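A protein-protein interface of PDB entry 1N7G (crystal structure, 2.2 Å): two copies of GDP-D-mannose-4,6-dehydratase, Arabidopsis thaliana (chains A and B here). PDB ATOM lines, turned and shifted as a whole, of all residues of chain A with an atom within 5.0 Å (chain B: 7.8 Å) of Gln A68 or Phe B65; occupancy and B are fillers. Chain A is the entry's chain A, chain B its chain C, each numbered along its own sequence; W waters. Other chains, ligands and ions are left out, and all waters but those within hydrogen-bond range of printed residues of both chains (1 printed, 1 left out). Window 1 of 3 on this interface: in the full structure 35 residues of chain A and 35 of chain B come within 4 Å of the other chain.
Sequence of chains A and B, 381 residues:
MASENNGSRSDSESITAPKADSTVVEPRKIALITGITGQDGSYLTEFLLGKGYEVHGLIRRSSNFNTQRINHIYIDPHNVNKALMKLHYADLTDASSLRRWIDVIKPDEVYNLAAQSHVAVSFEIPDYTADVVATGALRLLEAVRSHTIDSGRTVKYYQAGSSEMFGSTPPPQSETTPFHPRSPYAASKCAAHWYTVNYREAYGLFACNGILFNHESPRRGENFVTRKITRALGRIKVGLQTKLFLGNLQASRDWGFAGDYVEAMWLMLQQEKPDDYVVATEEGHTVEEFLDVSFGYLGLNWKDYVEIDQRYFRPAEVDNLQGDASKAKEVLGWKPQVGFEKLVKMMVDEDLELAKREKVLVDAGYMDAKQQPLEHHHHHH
The side-chain amide oxygen (OE1) of Gln B68 sits close to the backbone carbonyl oxygen (O) of Asn B66 (3.5 Å). The backbone carbonyl oxygen of Phe A65 sits at hydrogen-bond distance from the side-chain amide nitrogen of Gln A68. The side-chain hydroxyl of Ser B62 is in hydrogen-bond range of the backbone carbonyl oxygen of Asn B64 (2.4 Å). NE2 of Gln B68 sits at hydrogen-bond distance from O of Phe B65. The backbone carbonyl oxygen (O) of Asn A66 sits close to the side-chain amide oxygen (OE1) of Gln A68 (3.4 Å).
Along chain A the printed residues that touch a printed residue of chain B span positions 65 to 69. Among the printed residues, no Asp or Glu carboxylate lies within 4 Å of a Lys or Arg side-chain nitrogen of the other chain.
Water W1 bridges NH1 of Arg A69 (3.1 Å) and O of Ser B63 (3.3 Å).
The backbone carbonyl oxygen (O) of Ser B63 sits at hydrogen-bond distance from the guanidinium group (NH1) of Arg A69. The backbone carbonyl oxygen (O) of Asn A66 sits at hydrogen-bond distance from the side-chain amide nitrogen (ND2) of Asn B64, at 3.2 Å. NH2 of Arg A69 sits close to ND2 of Asn B64 (3.4 Å).
Of chain B, only Asn B64, Phe B65 and Gln B68 come within 4 Å of Gln A68. Printed residues of chain A within 4 Å of Phe B65: Gln A68. Of the printed residues of chain B, Phe A65 touches Gln B68 (3.9 Å). Printed residues of chain B within 4 Å of Arg A69: Ser B63 and Asn B64. Printed residues of chain A within 4 Å of Asn B64: Asn A66, Gln A68 and Arg A69. Thr A67 touches none of the printed residues of chain B. Asn B66 touches none of the printed residues of chain A. The nearest residue of chain A that does not touch Phe B65 is Phe A65 (4.3 Å). The nearest printed residue of chain A that does not touch Asn B64 is Thr A67 (4.7 Å).
Phe A65 touches Gln B68 (O to NE2, 3.9 Å). ND2 of Asn B64 touches OE1 of Gln A68, at 3.5 Å. Gln A68 touches Phe B65 (NE2 to O, 3.8 Å). Gln A68 touches Gln B68.
Phe A65 touches Gln B68, and with the chains exchanged Gln A68 touches Phe B65. Gln B68 touches its own counterpart, Gln A68. Of the 7 pairs that touch across the chains among the printed residues, 3 have their exchanged pair printed and touching as well.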
ATOM      1  N   PHE A  65     -32.553  24.645  -6.142  1.00  0.00           N
ATOM      2  CA  PHE A  65     -33.164  25.814  -5.522  1.00  0.00           C
ATOM      3  C   PHE A  65     -32.917  26.973  -6.494  1.00  0.00           C
ATOM      4  O   PHE A  65     -31.774  27.235  -6.866  1.00  0.00           O
ATOM      5  CB  PHE A  65     -32.460  26.061  -4.181  1.00  0.00           C
ATOM      6  CG  PHE A  65     -33.066  27.157  -3.344  1.00  0.00           C
ATOM      7  CD1 PHE A  65     -34.402  27.106  -2.953  1.00  0.00           C
ATOM      8  CD2 PHE A  65     -32.280  28.222  -2.907  1.00  0.00           C
ATOM      9  CE1 PHE A  65     -34.944  28.099  -2.137  1.00  0.00           C
ATOM     10  CE2 PHE A  65     -32.813  29.220  -2.089  1.00  0.00           C
ATOM     11  CZ  PHE A  65     -34.147  29.157  -1.705  1.00  0.00           C
ATOM     12  N   ASN A  66     -33.974  27.658  -6.921  1.00  0.00           N
ATOM     13  CA  ASN A  66     -33.801  28.766  -7.858  1.00  0.00           C
ATOM     14  C   ASN A  66     -34.422  30.080  -7.382  1.00  0.00           C
ATOM     15  O   ASN A  66     -34.497  31.047  -8.138  1.00  0.00           O
ATOM     16  CB  ASN A  66     -34.381  28.389  -9.225  1.00  0.00           C
ATOM     17  CG  ASN A  66     -35.898  28.381  -9.236  1.00  0.00           C
ATOM     18  OD1 ASN A  66     -36.541  27.897  -8.300  1.00  0.00           O
ATOM     19  ND2 ASN A  66     -36.479  28.907 -10.307  1.00  0.00           N
ATOM     20  N   THR A  67     -34.846  30.120  -6.124  1.00  0.00           N
ATOM     21  CA  THR A  67     -35.461  31.319  -5.573  1.00  0.00           C
ATOM     22  C   THR A  67     -34.586  32.000  -4.527  1.00  0.00           C
ATOM     23  O   THR A  67     -35.087  32.632  -3.605  1.00  0.00           O
ATOM     24  CB  THR A  67     -36.817  30.982  -4.945  1.00  0.00           C
ATOM     25  OG1 THR A  67     -36.656  29.903  -4.019  1.00  0.00           O
ATOM     26  CG2 THR A  67     -37.812  30.576  -6.024  1.00  0.00           C
ATOM     27  N   GLN A  68     -33.273  31.880  -4.684  1.00  0.00           N
ATOM     28  CA  GLN A  68     -32.338  32.476  -3.737  1.00  0.00           C
ATOM     29  C   GLN A  68     -32.535  33.971  -3.517  1.00  0.00           C
ATOM     30  O   GLN A  68     -32.309  34.463  -2.414  1.00  0.00           O
ATOM     31  CB  GLN A  68     -30.887  32.217  -4.173  1.00  0.00           C
ATOM     32  CG  GLN A  68     -30.483  30.737  -4.199  1.00  0.00           C
ATOM     33  CD  GLN A  68     -30.824  30.048  -5.513  1.00  0.00           C
ATOM     34  OE1 GLN A  68     -31.888  30.273  -6.084  1.00  0.00           O
ATOM     35  NE2 GLN A  68     -29.921  29.192  -5.990  1.00  0.00           N
ATOM     36  N   ARG A  69     -32.959  34.696  -4.550  1.00  0.00           N
ATOM     37  CA  ARG A  69     -33.149  36.142  -4.432  1.00  0.00           C
ATOM     38  C   ARG A  69     -34.445  36.601  -3.779  1.00  0.00           C
ATOM     39  O   ARG A  69     -34.530  37.733  -3.314  1.00  0.00           O
ATOM     40  CB  ARG A  69     -33.070  36.816  -5.799  1.00  0.00           C
ATOM     41  CG  ARG A  69     -31.722  36.774  -6.466  1.00  0.00           C
ATOM     42  CD  ARG A  69     -31.701  37.760  -7.618  1.00  0.00           C
ATOM     43  NE  ARG A  69     -30.475  37.660  -8.399  1.00  0.00           N
ATOM     44  CZ  ARG A  69     -30.268  36.757  -9.352  1.00  0.00           C
ATOM     45  NH1 ARG A  69     -29.116  36.743 -10.006  1.00  0.00           N
ATOM     46  NH2 ARG A  69     -31.216  35.881  -9.665  1.00  0.00           N
ATOM     47  N   ILE A  70     -35.455  35.741  -3.746  1.00  0.00           N
ATOM     48  CA  ILE A  70     -36.736  36.135  -3.172  1.00  0.00           C
ATOM     49  C   ILE A  70     -37.208  35.267  -2.013  1.00  0.00           C
ATOM     50  O   ILE A  70     -38.329  35.423  -1.540  1.00  0.00           O
ATOM     51  CB  ILE A  70     -37.833  36.146  -4.257  1.00  0.00           C
ATOM     52  CG1 ILE A  70     -37.966  34.752  -4.875  1.00  0.00           C
ATOM     53  CG2 ILE A  70     -37.498  37.184  -5.316  1.00  0.00           C
ATOM     54  CD1 ILE A  70     -38.980  34.657  -5.993  1.00  0.00           C
ATOM     55  N   ASN A  71     -36.357  34.359  -1.553  1.00  0.00           N
ATOM     56  CA  ASN A  71     -36.713  33.477  -0.449  1.00  0.00           C
ATOM     57  C   ASN A  71     -37.071  34.263   0.818  1.00  0.00           C
ATOM     58  O   ASN A  71     -38.024  33.924   1.515  1.00  0.00           O
ATOM     59  CB  ASN A  71     -35.557  32.523  -0.140  1.00  0.00           C
ATOM     60  CG  ASN A  71     -35.956  31.414   0.820  1.00  0.00           C
ATOM     61  OD1 ASN A  71     -35.130  30.906   1.582  1.00  0.00           O
ATOM     62  ND2 ASN A  71     -37.229  31.022   0.778  1.00  0.00           N
ATOM     63  N   ARG B  60     -28.392  24.488 -18.636  1.00  0.00           N
ATOM     64  CA  ARG B  60     -29.262  25.600 -18.970  1.00  0.00           C
ATOM     65  C   ARG B  60     -28.721  26.876 -18.352  1.00  0.00           C
ATOM     66  O   ARG B  60     -28.125  26.856 -17.275  1.00  0.00           O
ATOM     67  CB  ARG B  60     -30.676  25.384 -18.424  1.00  0.00           C
ATOM     68  CG  ARG B  60     -31.466  24.269 -19.064  1.00  0.00           C
ATOM     69  CD  ARG B  60     -32.936  24.407 -18.705  1.00  0.00           C
ATOM     70  NE  ARG B  60     -33.201  24.237 -17.276  1.00  0.00           N
ATOM     71  CZ  ARG B  60     -34.398  24.415 -16.721  1.00  0.00           C
ATOM     72  NH1 ARG B  60     -35.426  24.772 -17.478  1.00  0.00           N
ATOM     73  NH2 ARG B  60     -34.573  24.226 -15.414  1.00  0.00           N
ATOM     74  N   SER B  62     -29.153  30.128 -16.312  1.00  0.00           N
ATOM     75  CA  SER B  62     -30.106  30.500 -15.270  1.00  0.00           C
ATOM     76  C   SER B  62     -29.604  31.742 -14.557  1.00  0.00           C
ATOM     77  O   SER B  62     -28.403  31.988 -14.517  1.00  0.00           O
ATOM     78  CB  SER B  62     -30.293  29.358 -14.268  1.00  0.00           C
ATOM     79  OG  SER B  62     -29.103  29.119 -13.543  1.00  0.00           O
ATOM     80  N   SER B  63     -30.525  32.527 -14.002  1.00  0.00           N
ATOM     81  CA  SER B  63     -30.155  33.753 -13.305  1.00  0.00           C
ATOM     82  C   SER B  63     -29.450  33.444 -11.980  1.00  0.00           C
ATOM     83  O   SER B  63     -28.841  34.325 -11.369  1.00  0.00           O
ATOM     84  CB  SER B  63     -31.399  34.616 -13.052  1.00  0.00           C
ATOM     85  OG  SER B  63     -32.247  34.025 -12.082  1.00  0.00           O
ATOM     86  N   ASN B  64     -29.532  32.189 -11.550  1.00  0.00           N
ATOM     87  CA  ASN B  64     -28.896  31.755 -10.312  1.00  0.00           C
ATOM     88  C   ASN B  64     -27.958  30.581 -10.512  1.00  0.00           C
ATOM     89  O   ASN B  64     -27.956  29.938 -11.556  1.00  0.00           O
ATOM     90  CB  ASN B  64     -29.944  31.346  -9.280  1.00  0.00           C
ATOM     91  CG  ASN B  64     -30.521  32.520  -8.549  1.00  0.00           C
ATOM     92  OD1 ASN B  64     -29.791  33.282  -7.908  1.00  0.00           O
ATOM     93  ND2 ASN B  64     -31.835  32.680  -8.630  1.00  0.00           N
ATOM     94  N   PHE B  65     -27.166  30.318  -9.482  1.00  0.00           N
ATOM     95  CA  PHE B  65     -26.220  29.206  -9.445  1.00  0.00           C
ATOM     96  C   PHE B  65     -27.072  27.948  -9.681  1.00  0.00           C
ATOM     97  O   PHE B  65     -28.137  27.808  -9.076  1.00  0.00           O
ATOM     98  CB  PHE B  65     -25.574  29.199  -8.047  1.00  0.00           C
ATOM     99  CG  PHE B  65     -24.498  28.167  -7.850  1.00  0.00           C
ATOM    100  CD1 PHE B  65     -23.425  28.067  -8.733  1.00  0.00           C
ATOM    101  CD2 PHE B  65     -24.529  27.326  -6.734  1.00  0.00           C
ATOM    102  CE1 PHE B  65     -22.396  27.142  -8.507  1.00  0.00           C
ATOM    103  CE2 PHE B  65     -23.511  26.404  -6.500  1.00  0.00           C
ATOM    104  CZ  PHE B  65     -22.442  26.311  -7.389  1.00  0.00           C
ATOM    105  N   ASN B  66     -26.639  27.052 -10.566  1.00  0.00           N
ATOM    106  CA  ASN B  66     -27.415  25.836 -10.821  1.00  0.00           C
ATOM    107  C   ASN B  66     -26.563  24.574 -10.914  1.00  0.00           C
ATOM    108  O   ASN B  66     -27.036  23.526 -11.358  1.00  0.00           O
ATOM    109  CB  ASN B  66     -28.236  25.990 -12.101  1.00  0.00           C
ATOM    110  CG  ASN B  66     -27.381  25.963 -13.349  1.00  0.00           C
ATOM    111  OD1 ASN B  66     -26.249  26.451 -13.351  1.00  0.00           O
ATOM    112  ND2 ASN B  66     -27.923  25.405 -14.424  1.00  0.00           N
ATOM    113  N   THR B  67     -25.310  24.675 -10.482  1.00  0.00           N
ATOM    114  CA  THR B  67     -24.394  23.543 -10.519  1.00  0.00           C
ATOM    115  C   THR B  67     -24.030  23.061  -9.118  1.00  0.00           C
ATOM    116  O   THR B  67     -22.924  22.574  -8.889  1.00  0.00           O
ATOM    117  CB  THR B  67     -23.101  23.912 -11.262  1.00  0.00           C
ATOM    118  OG1 THR B  67     -22.562  25.122 -10.710  1.00  0.00           O
ATOM    119  CG2 THR B  67     -23.373  24.109 -12.745  1.00  0.00           C
ATOM    120  N   GLN B  68     -24.966  23.188  -8.187  1.00  0.00           N
ATOM    121  CA  GLN B  68     -24.734  22.773  -6.811  1.00  0.00           C
ATOM    122  C   GLN B  68     -24.270  21.331  -6.657  1.00  0.00           C
ATOM    123  O   GLN B  68     -23.391  21.047  -5.845  1.00  0.00           O
ATOM    124  CB  GLN B  68     -25.994  22.987  -5.964  1.00  0.00           C
ATOM    125  CG  GLN B  68     -26.361  24.446  -5.763  1.00  0.00           C
ATOM    126  CD  GLN B  68     -27.221  25.005  -6.884  1.00  0.00           C
ATOM    127  OE1 GLN B  68     -27.071  24.633  -8.047  1.00  0.00           O
ATOM    128  NE2 GLN B  68     -28.126  25.916  -6.533  1.00  0.00           N
ATOM    129  N   ARG B  69     -24.854  20.420  -7.433  1.00  0.00           N
ATOM    130  CA  ARG B  69     -24.501  19.002  -7.343  1.00  0.00           C
ATOM    131  C   ARG B  69     -23.175  18.598  -7.977  1.00  0.00           C
ATOM    132  O   ARG B  69     -22.626  17.548  -7.639  1.00  0.00           O
ATOM    133  CB  ARG B  69     -25.597  18.131  -7.965  1.00  0.00           C
ATOM    134  CG  ARG B  69     -26.949  18.208  -7.287  1.00  0.00           C
ATOM    135  CD  ARG B  69     -27.882  17.129  -7.815  1.00  0.00           C
ATOM    136  NE  ARG B  69     -29.240  17.313  -7.317  1.00  0.00           N
ATOM    137  CZ  ARG B  69     -30.143  18.112  -7.878  1.00  0.00           C
ATOM    138  NH1 ARG B  69     -31.351  18.222  -7.347  1.00  0.00           N
ATOM    139  NH2 ARG B  69     -29.844  18.784  -8.980  1.00  0.00           N
ATOM    140  N   ILE B  70     -22.652  19.410  -8.888  1.00  0.00           N
ATOM    141  CA  ILE B  70     -21.413  19.043  -9.561  1.00  0.00           C
ATOM    142  C   ILE B  70     -20.231  19.972  -9.353  1.00  0.00           C
ATOM    143  O   ILE B  70     -19.129  19.689  -9.824  1.00  0.00           O
ATOM    144  CB  ILE B  70     -21.640  18.905 -11.074  1.00  0.00           C
ATOM    145  CG1 ILE B  70     -22.162  20.227 -11.640  1.00  0.00           C
ATOM    146  CG2 ILE B  70     -22.620  17.781 -11.346  1.00  0.00           C
ATOM    147  CD1 ILE B  70     -22.307  20.226 -13.142  1.00  0.00           C
ATOM    148  N   ASN B  71     -20.451  21.073  -8.647  1.00  0.00           N
ATOM    149  CA  ASN B  71     -19.384  22.029  -8.409  1.00  0.00           C
ATOM    150  C   ASN B  71     -18.160  21.408  -7.734  1.00  0.00           C
ATOM    151  O   ASN B  71     -17.029  21.797  -8.020  1.00  0.00           O
ATOM    152  CB  ASN B  71     -19.909  23.200  -7.574  1.00  0.00           C
ATOM    153  CG  ASN B  71     -18.888  24.305  -7.425  1.00  0.00           C
ATOM    154  OD1 ASN B  71     -18.007  24.244  -6.565  1.00  0.00           O
ATOM    155  ND2 ASN B  71     -18.986  25.318  -8.279  1.00  0.00           N
ATOM    156  N   HIS B  72     -18.393  20.437  -6.854  1.00  0.00           N
ATOM    157  CA  HIS B  72     -17.314  19.760  -6.138  1.00  0.00           C
ATOM    158  C   HIS B  72     -16.480  18.855  -7.044  1.00  0.00           C
ATOM    159  O   HIS B  72     -15.317  18.577  -6.749  1.00  0.00           O
ATOM    160  CB  HIS B  72     -17.875  18.900  -5.008  1.00  0.00           C
ATOM    161  CG  HIS B  72     -18.547  17.651  -5.484  1.00  0.00           C
ATOM    162  ND1 HIS B  72     -19.787  17.654  -6.087  1.00  0.00           N
ATOM    163  CD2 HIS B  72     -18.139  16.359  -5.470  1.00  0.00           C
ATOM    164  CE1 HIS B  72     -20.116  16.417  -6.420  1.00  0.00           C
ATOM    165  NE2 HIS B  72     -19.132  15.612  -6.056  1.00  0.00           N
ATOM    166  N   TYR B  74     -14.963  19.443  -9.362  1.00  0.00           N
ATOM    167  CA  TYR B  74     -13.767  20.141  -9.808  1.00  0.00           C
ATOM    168  C   TYR B  74     -12.598  19.839  -8.860  1.00  0.00           C
ATOM    169  O   TYR B  74     -11.511  19.466  -9.301  1.00  0.00           O
ATOM    170  CB  TYR B  74     -14.022  21.646  -9.863  1.00  0.00           C
ATOM    171  CG  TYR B  74     -14.968  22.072 -10.962  1.00  0.00           C
ATOM    172  CD1 TYR B  74     -14.665  21.831 -12.303  1.00  0.00           C
ATOM    173  CD2 TYR B  74     -16.153  22.748 -10.666  1.00  0.00           C
ATOM    174  CE1 TYR B  74     -15.518  22.261 -13.325  1.00  0.00           C
ATOM    175  CE2 TYR B  74     -17.011  23.180 -11.676  1.00  0.00           C
ATOM    176  CZ  TYR B  74     -16.687  22.937 -13.001  1.00  0.00           C
ATOM    177  OH  TYR B  74     -17.519  23.388 -14.000  1.00  0.00           O
HETATM  178  O   HOH W   1     -28.742  37.188 -13.091  1.00  0.00           O
